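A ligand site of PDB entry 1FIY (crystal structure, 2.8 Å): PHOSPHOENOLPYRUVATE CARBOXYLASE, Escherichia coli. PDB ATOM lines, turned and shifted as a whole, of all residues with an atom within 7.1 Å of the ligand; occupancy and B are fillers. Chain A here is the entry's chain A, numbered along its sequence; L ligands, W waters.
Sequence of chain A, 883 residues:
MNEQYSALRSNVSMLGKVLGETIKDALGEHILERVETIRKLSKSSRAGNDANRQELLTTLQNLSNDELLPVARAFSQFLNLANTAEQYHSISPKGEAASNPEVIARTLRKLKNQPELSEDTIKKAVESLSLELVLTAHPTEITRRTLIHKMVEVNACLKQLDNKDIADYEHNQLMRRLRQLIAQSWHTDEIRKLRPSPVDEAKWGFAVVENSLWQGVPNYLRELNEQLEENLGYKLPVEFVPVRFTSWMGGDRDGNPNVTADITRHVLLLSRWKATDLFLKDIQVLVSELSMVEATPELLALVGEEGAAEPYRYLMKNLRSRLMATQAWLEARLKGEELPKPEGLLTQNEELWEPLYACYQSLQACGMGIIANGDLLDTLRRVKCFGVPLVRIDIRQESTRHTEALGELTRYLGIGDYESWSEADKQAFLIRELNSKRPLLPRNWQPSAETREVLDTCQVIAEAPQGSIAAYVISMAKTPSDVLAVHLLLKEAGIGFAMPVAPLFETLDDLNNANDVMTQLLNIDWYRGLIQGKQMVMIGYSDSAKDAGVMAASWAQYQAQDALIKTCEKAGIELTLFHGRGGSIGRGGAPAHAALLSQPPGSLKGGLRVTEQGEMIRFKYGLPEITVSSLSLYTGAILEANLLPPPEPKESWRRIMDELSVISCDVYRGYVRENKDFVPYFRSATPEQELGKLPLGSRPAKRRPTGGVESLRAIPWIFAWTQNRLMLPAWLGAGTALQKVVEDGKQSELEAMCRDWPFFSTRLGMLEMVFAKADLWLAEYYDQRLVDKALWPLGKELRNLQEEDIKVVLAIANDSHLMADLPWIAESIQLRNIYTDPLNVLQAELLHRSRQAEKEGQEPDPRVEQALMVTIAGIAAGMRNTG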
ATOM      1  N   ASN A  83     -32.367   0.783  11.589  1.00  0.00           N
ATOM      2  CA  ASN A  83     -31.187   0.424  12.388  1.00  0.00           C
ATOM      3  C   ASN A  83     -31.412   0.666  13.878  1.00  0.00           C
ATOM      4  O   ASN A  83     -30.885  -0.069  14.704  1.00  0.00           O
ATOM      5  CB  ASN A  83     -29.960   1.208  11.976  1.00  0.00           C
ATOM      6  CG  ASN A  83     -29.194   0.764  10.771  1.00  0.00           C
ATOM      7  OD1 ASN A  83     -28.804  -0.408  10.623  1.00  0.00           O
ATOM      8  ND2 ASN A  83     -28.920   1.735   9.882  1.00  0.00           N
ATOM      9  N   GLU A  86     -33.466  -2.013  15.081  1.00  0.00           N
ATOM     10  CA  GLU A  86     -32.552  -3.156  15.135  1.00  0.00           C
ATOM     11  C   GLU A  86     -31.614  -3.126  16.324  1.00  0.00           C
ATOM     12  O   GLU A  86     -31.491  -4.114  17.052  1.00  0.00           O
ATOM     13  CB  GLU A  86     -31.798  -3.271  13.820  1.00  0.00           C
ATOM     14  CG  GLU A  86     -31.213  -4.646  13.537  1.00  0.00           C
ATOM     15  CD  GLU A  86     -29.744  -4.652  13.891  1.00  0.00           C
ATOM     16  OE1 GLU A  86     -29.207  -3.537  14.113  1.00  0.00           O
ATOM     17  OE2 GLU A  86     -29.105  -5.717  13.940  1.00  0.00           O
ATOM     18  N   GLY A 583     -11.975  -7.253   7.899  1.00  0.00           N
ATOM     19  CA  GLY A 583     -11.559  -8.668   8.111  1.00  0.00           C
ATOM     20  C   GLY A 583     -12.617  -9.325   8.993  1.00  0.00           C
ATOM     21  O   GLY A 583     -13.716  -8.792   9.211  1.00  0.00           O
ATOM     22  N   SER A 584     -12.302 -10.487   9.541  1.00  0.00           N
ATOM     23  CA  SER A 584     -13.280 -11.207  10.356  1.00  0.00           C
ATOM     24  C   SER A 584     -13.177 -10.777  11.799  1.00  0.00           C
ATOM     25  O   SER A 584     -14.125 -10.972  12.579  1.00  0.00           O
ATOM     26  CB  SER A 584     -13.176 -12.699  10.072  1.00  0.00           C
ATOM     27  OG  SER A 584     -12.209 -13.335  10.876  1.00  0.00           O
ATOM     28  N   GLY A 586     -12.970  -7.642  12.652  1.00  0.00           N
ATOM     29  CA  GLY A 586     -13.734  -6.417  12.800  1.00  0.00           C
ATOM     30  C   GLY A 586     -15.201  -6.578  12.485  1.00  0.00           C
ATOM     31  O   GLY A 586     -15.878  -5.617  12.091  1.00  0.00           O
ATOM     32  N   ARG A 587     -15.709  -7.799  12.661  1.00  0.00           N
ATOM     33  CA  ARG A 587     -17.088  -8.132  12.345  1.00  0.00           C
ATOM     34  C   ARG A 587     -18.040  -7.705  13.466  1.00  0.00           C
ATOM     35  O   ARG A 587     -19.216  -7.435  13.219  1.00  0.00           O
ATOM     36  CB  ARG A 587     -17.232  -9.658  12.135  1.00  0.00           C
ATOM     37  CG  ARG A 587     -16.666 -10.134  10.813  1.00  0.00           C
ATOM     38  CD  ARG A 587     -17.010 -11.538  10.421  1.00  0.00           C
ATOM     39  NE  ARG A 587     -18.426 -11.807  10.300  1.00  0.00           N
ATOM     40  CZ  ARG A 587     -19.030 -12.930   9.967  1.00  0.00           C
ATOM     41  NH1 ARG A 587     -18.355 -14.032   9.688  1.00  0.00           N
ATOM     42  NH2 ARG A 587     -20.344 -12.974   9.886  1.00  0.00           N
ATOM     43  N   GLY A 588     -17.491  -7.674  14.677  1.00  0.00           N
ATOM     44  CA  GLY A 588     -18.296  -7.312  15.829  1.00  0.00           C
ATOM     45  C   GLY A 588     -19.070  -8.569  16.248  1.00  0.00           C
ATOM     46  O   GLY A 588     -19.134  -9.538  15.502  1.00  0.00           O
ATOM     47  N   GLY A 589     -19.589  -8.562  17.464  1.00  0.00           N
ATOM     48  CA  GLY A 589     -20.370  -9.610  18.000  1.00  0.00           C
ATOM     49  C   GLY A 589     -19.803 -11.001  18.003  1.00  0.00           C
ATOM     50  O   GLY A 589     -18.607 -11.246  18.130  1.00  0.00           O
ATOM     51  N   PRO A 591     -19.449 -13.318  15.651  1.00  0.00           N
ATOM     52  CA  PRO A 591     -18.442 -13.638  14.651  1.00  0.00           C
ATOM     53  C   PRO A 591     -17.064 -13.204  15.094  1.00  0.00           C
ATOM     54  O   PRO A 591     -16.124 -13.982  14.937  1.00  0.00           O
ATOM     55  CB  PRO A 591     -18.944 -12.991  13.375  1.00  0.00           C
ATOM     56  CG  PRO A 591     -20.433 -12.902  13.588  1.00  0.00           C
ATOM     57  CD  PRO A 591     -20.581 -12.593  15.070  1.00  0.00           C
ATOM     58  N   ALA A 592     -16.931 -12.007  15.695  1.00  0.00           N
ATOM     59  CA  ALA A 592     -15.633 -11.536  16.144  1.00  0.00           C
ATOM     60  C   ALA A 592     -15.084 -12.471  17.212  1.00  0.00           C
ATOM     61  O   ALA A 592     -13.913 -12.859  17.121  1.00  0.00           O
ATOM     62  CB  ALA A 592     -15.644 -10.120  16.626  1.00  0.00           C
ATOM     63  N   MET A 616     -18.391   1.442  11.809  1.00  0.00           N
ATOM     64  CA  MET A 616     -18.981   0.492  12.723  1.00  0.00           C
ATOM     65  C   MET A 616     -19.105   1.000  14.145  1.00  0.00           C
ATOM     66  O   MET A 616     -19.633   0.319  15.016  1.00  0.00           O
ATOM     67  CB  MET A 616     -18.170  -0.823  12.709  1.00  0.00           C
ATOM     68  CG  MET A 616     -18.359  -1.609  11.413  1.00  0.00           C
ATOM     69  SD  MET A 616     -20.054  -2.243  11.249  1.00  0.00           S
ATOM     70  CE  MET A 616     -19.946  -3.509  12.537  1.00  0.00           C
ATOM     71  N   PHE A 619     -22.563   0.876  15.620  1.00  0.00           N
ATOM     72  CA  PHE A 619     -22.950  -0.504  15.862  1.00  0.00           C
ATOM     73  C   PHE A 619     -22.130  -1.207  16.893  1.00  0.00           C
ATOM     74  O   PHE A 619     -22.582  -2.211  17.483  1.00  0.00           O
ATOM     75  CB  PHE A 619     -23.066  -1.168  14.499  1.00  0.00           C
ATOM     76  CG  PHE A 619     -23.912  -0.318  13.562  1.00  0.00           C
ATOM     77  CD1 PHE A 619     -25.230  -0.034  13.859  1.00  0.00           C
ATOM     78  CD2 PHE A 619     -23.374   0.194  12.399  1.00  0.00           C
ATOM     79  CE1 PHE A 619     -26.005   0.732  13.016  1.00  0.00           C
ATOM     80  CE2 PHE A 619     -24.139   0.965  11.543  1.00  0.00           C
ATOM     81  CZ  PHE A 619     -25.463   1.241  11.840  1.00  0.00           C
ATOM     82  N   MET A 766     -17.196 -15.614   6.856  1.00  0.00           N
ATOM     83  CA  MET A 766     -17.010 -14.311   6.289  1.00  0.00           C
ATOM     84  C   MET A 766     -17.420 -14.181   4.857  1.00  0.00           C
ATOM     85  O   MET A 766     -17.928 -13.086   4.553  1.00  0.00           O
ATOM     86  CB  MET A 766     -15.538 -13.909   6.451  1.00  0.00           C
ATOM     87  CG  MET A 766     -15.084 -12.564   5.957  1.00  0.00           C
ATOM     88  SD  MET A 766     -15.546 -11.212   7.110  1.00  0.00           S
ATOM     89  CE  MET A 766     -15.783  -9.933   5.848  1.00  0.00           C
ATOM     90  N   MET A 769     -21.466 -13.864   4.743  1.00  0.00           N
ATOM     91  CA  MET A 769     -22.011 -12.574   5.141  1.00  0.00           C
ATOM     92  C   MET A 769     -21.884 -11.623   3.968  1.00  0.00           C
ATOM     93  O   MET A 769     -22.863 -10.970   3.589  1.00  0.00           O
ATOM     94  CB  MET A 769     -21.364 -12.048   6.405  1.00  0.00           C
ATOM     95  CG  MET A 769     -21.733 -10.629   6.790  1.00  0.00           C
ATOM     96  SD  MET A 769     -20.350  -9.476   6.661  1.00  0.00           S
ATOM     97  CE  MET A 769     -20.599  -8.781   5.051  1.00  0.00           C
ATOM     98  N   VAL A 770     -20.713 -11.619   3.332  1.00  0.00           N
ATOM     99  CA  VAL A 770     -20.527 -10.753   2.160  1.00  0.00           C
ATOM    100  C   VAL A 770     -21.519 -11.124   1.078  1.00  0.00           C
ATOM    101  O   VAL A 770     -22.129 -10.262   0.447  1.00  0.00           O
ATOM    102  CB  VAL A 770     -19.080 -10.841   1.623  1.00  0.00           C
ATOM    103  CG1 VAL A 770     -18.940 -10.101   0.298  1.00  0.00           C
ATOM    104  CG2 VAL A 770     -18.091 -10.250   2.614  1.00  0.00           C
ATOM    105  N   LYS A 773     -25.050  -9.814   1.837  1.00  0.00           N
ATOM    106  CA  LYS A 773     -25.359  -8.419   1.595  1.00  0.00           C
ATOM    107  C   LYS A 773     -25.220  -8.046   0.112  1.00  0.00           C
ATOM    108  O   LYS A 773     -25.865  -7.083  -0.326  1.00  0.00           O
ATOM    109  CB  LYS A 773     -24.509  -7.460   2.421  1.00  0.00           C
ATOM    110  CG  LYS A 773     -24.475  -7.715   3.900  1.00  0.00           C
ATOM    111  CD  LYS A 773     -23.328  -6.950   4.560  1.00  0.00           C
ATOM    112  CE  LYS A 773     -23.619  -6.821   6.040  1.00  0.00           C
ATOM    113  NZ  LYS A 773     -22.501  -6.380   6.902  1.00  0.00           N
ATOM    114  N   MET A 819     -25.187 -18.256   5.751  1.00  0.00           N
ATOM    115  CA  MET A 819     -25.070 -17.799   7.131  1.00  0.00           C
ATOM    116  C   MET A 819     -26.277 -18.261   7.945  1.00  0.00           C
ATOM    117  O   MET A 819     -27.006 -17.517   8.578  1.00  0.00           O
ATOM    118  CB  MET A 819     -24.726 -16.339   7.221  1.00  0.00           C
ATOM    119  CG  MET A 819     -25.750 -15.262   7.185  1.00  0.00           C
ATOM    120  SD  MET A 819     -25.029 -13.625   7.034  1.00  0.00           S
ATOM    121  CE  MET A 819     -24.520 -13.277   8.721  1.00  0.00           C
ATOM    122  N   LEU A 822     -26.231 -18.161  12.046  1.00  0.00           N
ATOM    123  CA  LEU A 822     -26.482 -16.878  12.682  1.00  0.00           C
ATOM    124  C   LEU A 822     -27.801 -16.287  12.203  1.00  0.00           C
ATOM    125  O   LEU A 822     -27.844 -15.373  11.373  1.00  0.00           O
ATOM    126  CB  LEU A 822     -25.344 -15.912  12.428  1.00  0.00           C
ATOM    127  CG  LEU A 822     -23.916 -16.231  12.871  1.00  0.00           C
ATOM    128  CD1 LEU A 822     -22.911 -15.695  11.841  1.00  0.00           C
ATOM    129  CD2 LEU A 822     -23.585 -15.649  14.236  1.00  0.00           C
ATOM    130  N   ILE A 825     -28.344 -12.228  12.982  1.00  0.00           N
ATOM    131  CA  ILE A 825     -27.569 -11.460  12.008  1.00  0.00           C
ATOM    132  C   ILE A 825     -28.140 -11.648  10.607  1.00  0.00           C
ATOM    133  O   ILE A 825     -28.253 -10.680   9.848  1.00  0.00           O
ATOM    134  CB  ILE A 825     -26.064 -11.718  12.059  1.00  0.00           C
ATOM    135  CG1 ILE A 825     -25.531 -11.526  13.486  1.00  0.00           C
ATOM    136  CG2 ILE A 825     -25.326 -10.756  11.120  1.00  0.00           C
ATOM    137  CD1 ILE A 825     -24.171 -12.132  13.738  1.00  0.00           C
ATOM    138  N   ALA A 826     -28.541 -12.881  10.272  1.00  0.00           N
ATOM    139  CA  ALA A 826     -29.160 -13.122   8.959  1.00  0.00           C
ATOM    140  C   ALA A 826     -30.419 -12.278   8.827  1.00  0.00           C
ATOM    141  O   ALA A 826     -30.602 -11.582   7.829  1.00  0.00           O
ATOM    142  CB  ALA A 826     -29.488 -14.592   8.762  1.00  0.00           C
ATOM    143  N   SER A 828     -31.431  -9.560  10.587  1.00  0.00           N
ATOM    144  CA  SER A 828     -31.080  -8.142  10.575  1.00  0.00           C
ATOM    145  C   SER A 828     -30.540  -7.730   9.208  1.00  0.00           C
ATOM    146  O   SER A 828     -30.895  -6.651   8.705  1.00  0.00           O
ATOM    147  CB  SER A 828     -30.094  -7.856  11.689  1.00  0.00           C
ATOM    148  OG  SER A 828     -29.175  -6.829  11.330  1.00  0.00           O
ATOM    149  N   ILE A 829     -29.753  -8.569   8.539  1.00  0.00           N
ATOM    150  CA  ILE A 829     -29.246  -8.247   7.213  1.00  0.00           C
ATOM    151  C   ILE A 829     -30.412  -8.202   6.232  1.00  0.00           C
ATOM    152  O   ILE A 829     -30.473  -7.387   5.336  1.00  0.00           O
ATOM    153  CB  ILE A 829     -28.190  -9.238   6.716  1.00  0.00           C
ATOM    154  CG1 ILE A 829     -26.822  -9.056   7.419  1.00  0.00           C
ATOM    155  CG2 ILE A 829     -27.941  -9.154   5.212  1.00  0.00           C
ATOM    156  CD1 ILE A 829     -25.997 -10.318   7.383  1.00  0.00           C
ATOM    157  N   ARG A 832     -32.363  -4.694   6.675  1.00  0.00           N
ATOM    158  CA  ARG A 832     -31.595  -3.584   6.129  1.00  0.00           C
ATOM    159  C   ARG A 832     -31.519  -3.632   4.625  1.00  0.00           C
ATOM    160  O   ARG A 832     -31.583  -2.602   3.966  1.00  0.00           O
ATOM    161  CB  ARG A 832     -30.169  -3.572   6.677  1.00  0.00           C
ATOM    162  CG  ARG A 832     -30.109  -3.223   8.155  1.00  0.00           C
ATOM    163  CD  ARG A 832     -28.694  -3.253   8.619  1.00  0.00           C
ATOM    164  NE  ARG A 832     -28.346  -4.420   9.405  1.00  0.00           N
ATOM    165  CZ  ARG A 832     -27.251  -5.140   9.169  1.00  0.00           C
ATOM    166  NH1 ARG A 832     -26.447  -4.777   8.169  1.00  0.00           N
ATOM    167  NH2 ARG A 832     -26.976  -6.185   9.927  1.00  0.00           N
ATOM    168  N   ALA A 877     -24.561   2.912   5.679  1.00  0.00           N
ATOM    169  CA  ALA A 877     -25.139   2.658   7.005  1.00  0.00           C
ATOM    170  C   ALA A 877     -25.887   1.336   7.091  1.00  0.00           C
ATOM    171  O   ALA A 877     -25.785   0.640   8.094  1.00  0.00           O
ATOM    172  CB  ALA A 877     -26.027   3.811   7.404  1.00  0.00           C
ATOM    173  N   GLY A 878     -26.627   1.020   6.038  1.00  0.00           N
ATOM    174  CA  GLY A 878     -27.378  -0.207   5.911  1.00  0.00           C
ATOM    175  C   GLY A 878     -26.460  -1.413   5.739  1.00  0.00           C
ATOM    176  O   GLY A 878     -26.688  -2.416   6.406  1.00  0.00           O
ATOM    177  N   MET A 879     -25.387  -1.279   4.943  1.00  0.00           N
ATOM    178  CA  MET A 879     -24.453  -2.356   4.693  1.00  0.00           C
ATOM    179  C   MET A 879     -23.410  -2.586   5.761  1.00  0.00           C
ATOM    180  O   MET A 879     -22.784  -3.666   5.735  1.00  0.00           O
ATOM    181  CB  MET A 879     -23.709  -2.195   3.372  1.00  0.00           C
ATOM    182  CG  MET A 879     -24.618  -2.044   2.159  1.00  0.00           C
ATOM    183  SD  MET A 879     -25.771  -3.438   2.066  1.00  0.00           S
ATOM    184  CE  MET A 879     -24.978  -4.374   0.777  1.00  0.00           C
ATOM    185  N   ARG A 880     -23.164  -1.648   6.677  1.00  0.00           N
ATOM    186  CA  ARG A 880     -22.132  -1.868   7.686  1.00  0.00           C
ATOM    187  C   ARG A 880     -20.869  -2.460   7.079  1.00  0.00           C
ATOM    188  O   ARG A 880     -20.431  -2.075   6.013  1.00  0.00           O
ATOM    189  CB  ARG A 880     -22.656  -2.747   8.817  1.00  0.00           C
ATOM    190  CG  ARG A 880     -23.842  -2.051   9.493  1.00  0.00           C
ATOM    191  CD  ARG A 880     -24.611  -2.976  10.398  1.00  0.00           C
ATOM    192  NE  ARG A 880     -25.930  -2.398  10.703  1.00  0.00           N
ATOM    193  CZ  ARG A 880     -26.518  -2.705  11.864  1.00  0.00           C
ATOM    194  NH1 ARG A 880     -25.842  -3.520  12.672  1.00  0.00           N
ATOM    195  NH2 ARG A 880     -27.693  -2.190  12.168  1.00  0.00           N
ATOM    196  N   ASN A 881     -20.260  -3.398   7.788  1.00  0.00           N
ATOM    197  CA  ASN A 881     -19.045  -4.045   7.367  1.00  0.00           C
ATOM    198  C   ASN A 881     -19.225  -4.992   6.187  1.00  0.00           C
ATOM    199  O   ASN A 881     -20.001  -5.933   6.138  1.00  0.00           O
ATOM    200  CB  ASN A 881     -18.390  -4.735   8.557  1.00  0.00           C
ATOM    201  CG  ASN A 881     -19.167  -5.951   8.988  1.00  0.00           C
ATOM    202  OD1 ASN A 881     -20.401  -5.894   9.007  1.00  0.00           O
ATOM    203  ND2 ASN A 881     -18.460  -7.024   9.319  1.00  0.00           N
HETATM  204  N1  LIG L   1     -21.649  -7.511  11.507  1.00  0.00           N
HETATM  205  C1  LIG L   1     -22.509  -8.516  10.802  1.00  0.00           C
HETATM  206  C2  LIG L   1     -21.688  -9.664  10.253  1.00  0.00           C
HETATM  207  O1  LIG L   1     -22.182 -10.641   9.716  1.00  0.00           O
HETATM  208  C3  LIG L   1     -23.291  -7.829   9.688  1.00  0.00           C
HETATM  209  C4  LIG L   1     -24.148  -6.689  10.182  1.00  0.00           C
HETATM  210  O2  LIG L   1     -24.649  -6.720  11.337  1.00  0.00           O
HETATM  211  O3  LIG L   1     -24.322  -5.735   9.385  1.00  0.00           O
HETATM  212  O4  LIG L   1     -20.173  -9.651  10.290  1.00  0.00           O
HETATM  213  O   HOH W   1     -22.853  -5.356  13.336  1.00  0.00           O
HETATM  214  O   HOH W   2     -22.259  -8.880  13.982  1.00  0.00           O
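The guanidinium group (NH1) of Arg 832 lies within salt-bridge range of an oxygen (O3) of the ligand, 2.6 Å away.
A nitrogen (N1) of the ligand is in hydrogen-bond range of the backbone carbonyl oxygen (O) of Arg 587 (3.0 Å).
O4 of the ligand lies within salt-bridge range of NE of Arg 587 (2.8 Å).
The guanidinium group (NH1) of Arg 880 lies within salt-bridge range of an oxygen (O2) of the ligand, at 3.7 Å.
The side-chain amino group (NZ) of Lys 773 is in salt-bridge range of an oxygen (O3) of the ligand (3.1 Å).
N1 of the ligand lies within hydrogen-bond range of OD1 of Asn 881 (3.2 Å).
The guanidinium group of Arg 832 lies within hydrogen-bond range of the side-chain hydroxyl of Ser 828 (2.7 Å).
The guanidinium group (NH1) of Arg 832 sits at hydrogen-bond distance from the backbone carbonyl oxygen (O) of Gly 878 (3.0 Å).
The side-chain carboxylate of Glu 86 lies within salt-bridge range of the guanidinium group of Arg 880 (2.8 Å).
The guanidinium group of Arg 880 lies within hydrogen-bond range of the side-chain amide oxygen of Asn 83 (2.6 Å).
SD of Met 769 lies close to NZ of Lys 773 (3.8 Å).
The side-chain amino group of Lys 773 lies within hydrogen-bond range of the backbone carbonyl oxygen of Asn 881, 2.7 Å away.
The side-chain amino group (NZ) of Lys 773 lies within hydrogen-bond range of the backbone carbonyl oxygen (O) of Met 879.
The side-chain sulfur (SD) of Met 616 is in hydrogen-bond range of the backbone NH (N) of Asn 881, at 3.7 Å.
The side-chain sulfur (SD) of Met 769 lies close to an oxygen (O4) of the ligand (3.6 Å).
CE of Met 819 touches O1 of the ligand, at 3.7 Å.
CG2 of Ile 825 touches O1 of the ligand, 3.4 Å away.
Within 4 Å of the ligand: Arg 587, Met 769, Lys 773, Met 819, Ile 825, Arg 832, Arg 880 and Asn 881.
Water W2 bridges a nitrogen (N1) of the ligand (2.9 Å) and the backbone carbonyl oxygen (O) of Arg 587 (3.5 Å).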
